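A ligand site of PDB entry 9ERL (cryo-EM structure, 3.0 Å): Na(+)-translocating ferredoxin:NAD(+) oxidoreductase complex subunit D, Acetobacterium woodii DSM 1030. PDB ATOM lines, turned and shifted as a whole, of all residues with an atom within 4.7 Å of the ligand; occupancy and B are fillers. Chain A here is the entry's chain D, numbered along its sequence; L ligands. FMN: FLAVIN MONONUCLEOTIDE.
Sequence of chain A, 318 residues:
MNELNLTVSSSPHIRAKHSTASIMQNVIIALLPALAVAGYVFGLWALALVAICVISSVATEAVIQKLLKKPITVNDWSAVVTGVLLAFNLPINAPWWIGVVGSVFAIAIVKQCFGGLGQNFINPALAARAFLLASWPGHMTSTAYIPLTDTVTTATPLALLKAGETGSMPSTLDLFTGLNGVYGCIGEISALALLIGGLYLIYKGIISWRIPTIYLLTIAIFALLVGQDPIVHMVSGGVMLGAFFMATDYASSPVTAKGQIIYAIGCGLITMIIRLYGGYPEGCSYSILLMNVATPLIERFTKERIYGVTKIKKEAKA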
ATOM      1  N   ASN A  89      14.032  17.706  -2.696  1.00  0.00           N
ATOM      2  CA  ASN A  89      13.801  18.959  -1.986  1.00  0.00           C
ATOM      3  C   ASN A  89      12.659  18.864  -0.981  1.00  0.00           C
ATOM      4  O   ASN A  89      11.992  19.872  -0.715  1.00  0.00           O
ATOM      5  CB  ASN A  89      13.507  20.084  -2.985  1.00  0.00           C
ATOM      6  CG  ASN A  89      14.766  20.651  -3.602  1.00  0.00           C
ATOM      7  OD1 ASN A  89      15.759  20.866  -2.922  1.00  0.00           O
ATOM      8  ND2 ASN A  89      14.724  20.907  -4.903  1.00  0.00           N
ATOM      9  N   LEU A 126      12.620  24.517  -8.513  1.00  0.00           N
ATOM     10  CA  LEU A 126      12.743  25.546  -7.475  1.00  0.00           C
ATOM     11  C   LEU A 126      11.474  26.369  -7.358  1.00  0.00           C
ATOM     12  O   LEU A 126      11.069  26.734  -6.248  1.00  0.00           O
ATOM     13  CB  LEU A 126      13.940  26.446  -7.772  1.00  0.00           C
ATOM     14  CG  LEU A 126      15.327  25.849  -7.514  1.00  0.00           C
ATOM     15  CD1 LEU A 126      16.410  26.876  -7.812  1.00  0.00           C
ATOM     16  CD2 LEU A 126      15.443  25.351  -6.083  1.00  0.00           C
ATOM     17  N   ARG A 129       9.004  24.275  -5.496  1.00  0.00           N
ATOM     18  CA  ARG A 129       9.353  24.252  -4.079  1.00  0.00           C
ATOM     19  C   ARG A 129       8.950  25.544  -3.386  1.00  0.00           C
ATOM     20  O   ARG A 129       8.431  25.518  -2.259  1.00  0.00           O
ATOM     21  CB  ARG A 129      10.856  24.018  -3.928  1.00  0.00           C
ATOM     22  CG  ARG A 129      11.275  23.665  -2.531  1.00  0.00           C
ATOM     23  CD  ARG A 129      12.679  24.144  -2.212  1.00  0.00           C
ATOM     24  NE  ARG A 129      13.117  23.609  -0.922  1.00  0.00           N
ATOM     25  CZ  ARG A 129      12.746  24.088   0.253  1.00  0.00           C
ATOM     26  NH1 ARG A 129      11.955  25.149   0.354  1.00  0.00           N
ATOM     27  NH2 ARG A 129      13.167  23.484   1.358  1.00  0.00           N
ATOM     28  N   SER A 142      10.918  23.217   9.732  1.00  0.00           N
ATOM     29  CA  SER A 142      11.667  23.074  10.980  1.00  0.00           C
ATOM     30  C   SER A 142      11.244  21.913  11.885  1.00  0.00           C
ATOM     31  O   SER A 142      11.913  21.650  12.887  1.00  0.00           O
ATOM     32  CB  SER A 142      11.588  24.371  11.785  1.00  0.00           C
ATOM     33  OG  SER A 142      10.460  24.372  12.646  1.00  0.00           O
ATOM     34  N   TYR A 145      11.467  17.925   9.222  1.00  0.00           N
ATOM     35  CA  TYR A 145      12.747  17.346   8.876  1.00  0.00           C
ATOM     36  C   TYR A 145      13.268  16.351   9.914  1.00  0.00           C
ATOM     37  O   TYR A 145      14.069  15.479   9.567  1.00  0.00           O
ATOM     38  CB  TYR A 145      13.775  18.459   8.661  1.00  0.00           C
ATOM     39  CG  TYR A 145      13.365  19.462   7.605  1.00  0.00           C
ATOM     40  CD1 TYR A 145      13.502  19.171   6.264  1.00  0.00           C
ATOM     41  CD2 TYR A 145      12.834  20.689   7.967  1.00  0.00           C
ATOM     42  CE1 TYR A 145      13.129  20.076   5.292  1.00  0.00           C
ATOM     43  CE2 TYR A 145      12.457  21.599   7.002  1.00  0.00           C
ATOM     44  CZ  TYR A 145      12.604  21.287   5.669  1.00  0.00           C
ATOM     45  OH  TYR A 145      12.226  22.197   4.704  1.00  0.00           O
ATOM     46  N   THR A 156      17.601  21.853  13.309  1.00  0.00           N
ATOM     47  CA  THR A 156      18.547  21.625  12.229  1.00  0.00           C
ATOM     48  C   THR A 156      19.722  22.588  12.348  1.00  0.00           C
ATOM     49  O   THR A 156      19.585  23.660  12.944  1.00  0.00           O
ATOM     50  CB  THR A 156      17.844  21.790  10.868  1.00  0.00           C
ATOM     51  OG1 THR A 156      17.862  23.199  10.457  1.00  0.00           O
ATOM     52  CG2 THR A 156      16.421  21.260  10.941  1.00  0.00           C
ATOM     53  N   LEU A 158      21.411  24.816  10.590  1.00  0.00           N
ATOM     54  CA  LEU A 158      21.333  26.212  10.167  1.00  0.00           C
ATOM     55  C   LEU A 158      20.517  27.066  11.123  1.00  0.00           C
ATOM     56  O   LEU A 158      20.871  28.225  11.358  1.00  0.00           O
ATOM     57  CB  LEU A 158      20.740  26.300   8.753  1.00  0.00           C
ATOM     58  CG  LEU A 158      21.723  26.279   7.587  1.00  0.00           C
ATOM     59  CD1 LEU A 158      21.000  26.592   6.287  1.00  0.00           C
ATOM     60  CD2 LEU A 158      22.866  27.247   7.809  1.00  0.00           C
ATOM     61  N   ALA A 159      19.436  26.523  11.685  1.00  0.00           N
ATOM     62  CA  ALA A 159      18.644  27.242  12.672  1.00  0.00           C
ATOM     63  C   ALA A 159      19.442  27.512  13.943  1.00  0.00           C
ATOM     64  O   ALA A 159      19.318  28.587  14.544  1.00  0.00           O
ATOM     65  CB  ALA A 159      17.368  26.467  12.995  1.00  0.00           C
ATOM     66  N   GLY A 184      17.673  17.134   7.596  1.00  0.00           N
ATOM     67  CA  GLY A 184      17.305  18.173   6.654  1.00  0.00           C
ATOM     68  C   GLY A 184      16.492  17.592   5.519  1.00  0.00           C
ATOM     69  O   GLY A 184      15.744  16.629   5.695  1.00  0.00           O
ATOM     70  N   CYS A 185      16.652  18.187   4.340  1.00  0.00           N
ATOM     71  CA  CYS A 185      16.078  17.602   3.140  1.00  0.00           C
ATOM     72  C   CYS A 185      16.766  16.264   2.852  1.00  0.00           C
ATOM     73  O   CYS A 185      17.937  16.064   3.167  1.00  0.00           O
ATOM     74  CB  CYS A 185      16.226  18.551   1.945  1.00  0.00           C
ATOM     75  SG  CYS A 185      15.277  20.076   2.091  1.00  0.00           S
ATOM     76  N   GLU A 188      20.202  16.318   0.560  1.00  0.00           N
ATOM     77  CA  GLU A 188      21.167  17.383   0.761  1.00  0.00           C
ATOM     78  C   GLU A 188      22.105  17.157   1.942  1.00  0.00           C
ATOM     79  O   GLU A 188      23.000  17.980   2.164  1.00  0.00           O
ATOM     80  CB  GLU A 188      20.443  18.724   0.967  1.00  0.00           C
ATOM     81  CG  GLU A 188      19.808  18.851   2.341  1.00  0.00           C
ATOM     82  CD  GLU A 188      19.813  20.270   2.871  1.00  0.00           C
ATOM     83  OE1 GLU A 188      19.667  21.207   2.067  1.00  0.00           O
ATOM     84  OE2 GLU A 188      19.981  20.452   4.101  1.00  0.00           O
ATOM     85  N   GLY A 237      23.286  23.107   4.628  1.00  0.00           N
ATOM     86  CA  GLY A 237      22.256  23.652   3.756  1.00  0.00           C
ATOM     87  C   GLY A 237      22.336  23.091   2.351  1.00  0.00           C
ATOM     88  O   GLY A 237      23.158  22.220   2.031  1.00  0.00           O
ATOM     89  N   GLY A 238      21.472  23.600   1.488  1.00  0.00           N
ATOM     90  CA  GLY A 238      21.427  23.154   0.113  1.00  0.00           C
ATOM     91  C   GLY A 238      22.284  23.975  -0.816  1.00  0.00           C
ATOM     92  O   GLY A 238      21.770  24.609  -1.751  1.00  0.00           O
ATOM     93  N   LEU A 241      24.278  20.922  -3.705  1.00  0.00           N
ATOM     94  CA  LEU A 241      23.279  20.490  -4.678  1.00  0.00           C
ATOM     95  C   LEU A 241      22.888  21.632  -5.598  1.00  0.00           C
ATOM     96  O   LEU A 241      22.796  21.452  -6.822  1.00  0.00           O
ATOM     97  CB  LEU A 241      22.049  19.944  -3.946  1.00  0.00           C
ATOM     98  CG  LEU A 241      20.966  19.283  -4.806  1.00  0.00           C
ATOM     99  CD1 LEU A 241      21.485  18.006  -5.447  1.00  0.00           C
ATOM    100  CD2 LEU A 241      19.719  19.019  -3.996  1.00  0.00           C
ATOM    101  N   GLY A 242      22.679  22.827  -5.043  1.00  0.00           N
ATOM    102  CA  GLY A 242      22.336  23.969  -5.875  1.00  0.00           C
ATOM    103  C   GLY A 242      23.472  24.378  -6.794  1.00  0.00           C
ATOM    104  O   GLY A 242      23.253  24.718  -7.951  1.00  0.00           O
ATOM    105  N   MET A 246      21.585  22.389  -9.765  1.00  0.00           N
ATOM    106  CA  MET A 246      20.421  23.242  -9.967  1.00  0.00           C
ATOM    107  C   MET A 246      20.742  24.615 -10.532  1.00  0.00           C
ATOM    108  O   MET A 246      19.858  25.205 -11.172  1.00  0.00           O
ATOM    109  CB  MET A 246      19.645  23.402  -8.654  1.00  0.00           C
ATOM    110  CG  MET A 246      19.491  22.108  -7.870  1.00  0.00           C
ATOM    111  SD  MET A 246      17.928  21.942  -6.990  1.00  0.00           S
ATOM    112  CE  MET A 246      16.772  22.048  -8.339  1.00  0.00           C
ATOM    113  N   TYR A 280      14.869  34.198   6.427  1.00  0.00           N
ATOM    114  CA  TYR A 280      14.940  32.763   6.184  1.00  0.00           C
ATOM    115  C   TYR A 280      16.273  32.229   6.699  1.00  0.00           C
ATOM    116  O   TYR A 280      17.258  32.974   6.755  1.00  0.00           O
ATOM    117  CB  TYR A 280      14.827  32.434   4.690  1.00  0.00           C
ATOM    118  CG  TYR A 280      13.554  32.890   4.020  1.00  0.00           C
ATOM    119  CD1 TYR A 280      12.410  32.110   4.039  1.00  0.00           C
ATOM    120  CD2 TYR A 280      13.499  34.102   3.341  1.00  0.00           C
ATOM    121  CE1 TYR A 280      11.242  32.524   3.426  1.00  0.00           C
ATOM    122  CE2 TYR A 280      12.349  34.525   2.719  1.00  0.00           C
ATOM    123  CZ  TYR A 280      11.224  33.735   2.772  1.00  0.00           C
ATOM    124  OH  TYR A 280      10.067  34.151   2.151  1.00  0.00           O
ATOM    125  N   PRO A 281      16.329  30.958   7.112  1.00  0.00           N
ATOM    126  CA  PRO A 281      17.624  30.361   7.451  1.00  0.00           C
ATOM    127  C   PRO A 281      18.500  30.067   6.248  1.00  0.00           C
ATOM    128  O   PRO A 281      19.709  29.849   6.418  1.00  0.00           O
ATOM    129  CB  PRO A 281      17.233  29.077   8.185  1.00  0.00           C
ATOM    130  CG  PRO A 281      15.900  28.739   7.641  1.00  0.00           C
ATOM    131  CD  PRO A 281      15.217  30.049   7.403  1.00  0.00           C
ATOM    132  N   GLU A 282      17.937  30.045   5.047  1.00  0.00           N
ATOM    133  CA  GLU A 282      18.650  29.714   3.820  1.00  0.00           C
ATOM    134  C   GLU A 282      18.056  30.529   2.684  1.00  0.00           C
ATOM    135  O   GLU A 282      16.848  30.767   2.639  1.00  0.00           O
ATOM    136  CB  GLU A 282      18.576  28.209   3.532  1.00  0.00           C
ATOM    137  CG  GLU A 282      19.116  27.767   2.173  1.00  0.00           C
ATOM    138  CD  GLU A 282      20.610  27.536   2.147  1.00  0.00           C
ATOM    139  OE1 GLU A 282      21.365  28.442   2.539  1.00  0.00           O
ATOM    140  OE2 GLU A 282      21.028  26.440   1.742  1.00  0.00           O
ATOM    141  N   GLY A 283      18.922  30.972   1.773  1.00  0.00           N
ATOM    142  CA  GLY A 283      18.460  31.755   0.648  1.00  0.00           C
ATOM    143  C   GLY A 283      18.978  31.320  -0.701  1.00  0.00           C
ATOM    144  O   GLY A 283      19.108  32.145  -1.621  1.00  0.00           O
ATOM    145  N   CYS A 284      19.281  30.032  -0.858  1.00  0.00           N
ATOM    146  CA  CYS A 284      19.829  29.532  -2.113  1.00  0.00           C
ATOM    147  C   CYS A 284      18.793  29.547  -3.229  1.00  0.00           C
ATOM    148  O   CYS A 284      19.080  29.974  -4.356  1.00  0.00           O
ATOM    149  CB  CYS A 284      20.369  28.112  -1.916  1.00  0.00           C
ATOM    150  SG  CYS A 284      21.323  27.468  -3.288  1.00  0.00           S
ATOM    151  N   SER A 285      17.572  29.094  -2.926  1.00  0.00           N
ATOM    152  CA  SER A 285      16.537  28.978  -3.946  1.00  0.00           C
ATOM    153  C   SER A 285      16.155  30.329  -4.536  1.00  0.00           C
ATOM    154  O   SER A 285      16.045  30.485  -5.752  1.00  0.00           O
ATOM    155  CB  SER A 285      15.305  28.291  -3.350  1.00  0.00           C
ATOM    156  OG  SER A 285      14.125  28.649  -4.042  1.00  0.00           O
ATOM    157  N   TYR A 286      15.980  31.331  -3.675  1.00  0.00           N
ATOM    158  CA  TYR A 286      15.599  32.659  -4.163  1.00  0.00           C
ATOM    159  C   TYR A 286      16.758  33.370  -4.825  1.00  0.00           C
ATOM    160  O   TYR A 286      16.543  34.176  -5.732  1.00  0.00           O
ATOM    161  CB  TYR A 286      15.035  33.488  -3.007  1.00  0.00           C
ATOM    162  CG  TYR A 286      13.860  32.833  -2.327  1.00  0.00           C
ATOM    163  CD1 TYR A 286      12.695  32.550  -3.028  1.00  0.00           C
ATOM    164  CD2 TYR A 286      13.904  32.502  -0.983  1.00  0.00           C
ATOM    165  CE1 TYR A 286      11.614  31.961  -2.419  1.00  0.00           C
ATOM    166  CE2 TYR A 286      12.835  31.906  -0.360  1.00  0.00           C
ATOM    167  CZ  TYR A 286      11.686  31.631  -1.085  1.00  0.00           C
ATOM    168  OH  TYR A 286      10.611  31.039  -0.469  1.00  0.00           O
HETATM  169  N1  FMN L   1      15.147  26.585   3.103  1.00  0.00           N
HETATM  170  C2  FMN L   1      14.679  27.846   3.199  1.00  0.00           C
HETATM  171  O2  FMN L   1      14.168  28.252   4.252  1.00  0.00           O
HETATM  172  N3  FMN L   1      14.728  28.721   2.162  1.00  0.00           N
HETATM  173  C4  FMN L   1      15.266  28.371   0.945  1.00  0.00           C
HETATM  174  O4  FMN L   1      15.303  29.186   0.043  1.00  0.00           O
HETATM  175  C4A FMN L   1      15.772  27.069   0.806  1.00  0.00           C
HETATM  176  N5  FMN L   1      16.287  26.723  -0.344  1.00  0.00           N
HETATM  177  C5A FMN L   1      16.769  25.446  -0.462  1.00  0.00           C
HETATM  178  C6  FMN L   1      17.331  25.060  -1.692  1.00  0.00           C
HETATM  179  C7  FMN L   1      17.830  23.794  -1.890  1.00  0.00           C
HETATM  180  C7M FMN L   1      18.419  23.419  -3.224  1.00  0.00           C
HETATM  181  C8  FMN L   1      17.789  22.864  -0.820  1.00  0.00           C
HETATM  182  C8M FMN L   1      18.329  21.472  -1.011  1.00  0.00           C
HETATM  183  C9  FMN L   1      17.242  23.235   0.388  1.00  0.00           C
HETATM  184  C9A FMN L   1      16.727  24.515   0.594  1.00  0.00           C
HETATM  185  N10 FMN L   1      16.166  24.925   1.808  1.00  0.00           N
HETATM  186  C10 FMN L   1      15.669  26.206   1.955  1.00  0.00           C
HETATM  187  C1' FMN L   1      16.113  23.990   2.943  1.00  0.00           C
HETATM  188  C2' FMN L   1      17.289  24.173   3.894  1.00  0.00           C
HETATM  189  O2' FMN L   1      18.511  23.944   3.195  1.00  0.00           O
HETATM  190  C3' FMN L   1      17.218  23.238   5.103  1.00  0.00           C
HETATM  191  O3' FMN L   1      17.252  21.893   4.655  1.00  0.00           O
HETATM  192  C4' FMN L   1      15.998  23.444   5.989  1.00  0.00           C
HETATM  193  O4' FMN L   1      15.966  24.791   6.465  1.00  0.00           O
HETATM  194  C5' FMN L   1      15.949  22.482   7.148  1.00  0.00           C
HETATM  195  O5' FMN L   1      17.075  22.597   8.074  1.00  0.00           O
HETATM  196  P   FMN L   1      17.068  23.776   9.182  1.00  0.00           P
HETATM  197  O1P FMN L   1      17.827  24.899   8.585  1.00  0.00           O
HETATM  198  O2P FMN L   1      15.648  24.000   9.544  1.00  0.00           O
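A nitrogen (N3) of the ligand is in hydrogen-bond range of the backbone carbonyl oxygen of Glu 282.
O2' of the ligand sits at hydrogen-bond distance from N of Gly 238.
An oxygen (O3') of the ligand is in hydrogen-bond range of the side-chain sulfur (SG) of Cys 185, at 3.7 Å.
A phosphorus (P) of the ligand is covalently linked to the side-chain hydroxyl (OG1) of Thr 156, at 1.6 Å.
The side-chain carboxylate of Glu 188 lies within hydrogen-bond range of an oxygen (O3') of the ligand (3.1 Å).
The guanidinium group of Arg 129 lies close to a nitrogen (N10) of the ligand (3.4 Å).
Residues that only touch the ligand: Asn 89, Tyr 145, Leu 158, Ala 159, Gly 237, Pro 281, Ser 285 and Tyr 286.
14 residues have an atom within 4 Å of the ligand: Asn 89, Arg 129, Tyr 145, Thr 156, Leu 158, Ala 159, Cys 185, Glu 188, Gly 237, Gly 238, Pro 281, Glu 282, Ser 285 and Tyr 286.
The nearest printed residue that does not touch the ligand is Met 246 (4.1 Å).
The backbone carbonyl oxygen (O) of Gly 238 lies within hydrogen-bond range of the side-chain sulfur (SG) of Cys 284 (3.3 Å).
N of Gly 238 sits at hydrogen-bond distance from OE2 of Glu 282 (2.9 Å).
The side-chain carboxylate (OE1) of Glu 188 lies within hydrogen-bond range of the backbone NH (N) of Gly 238 (3.1 Å).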
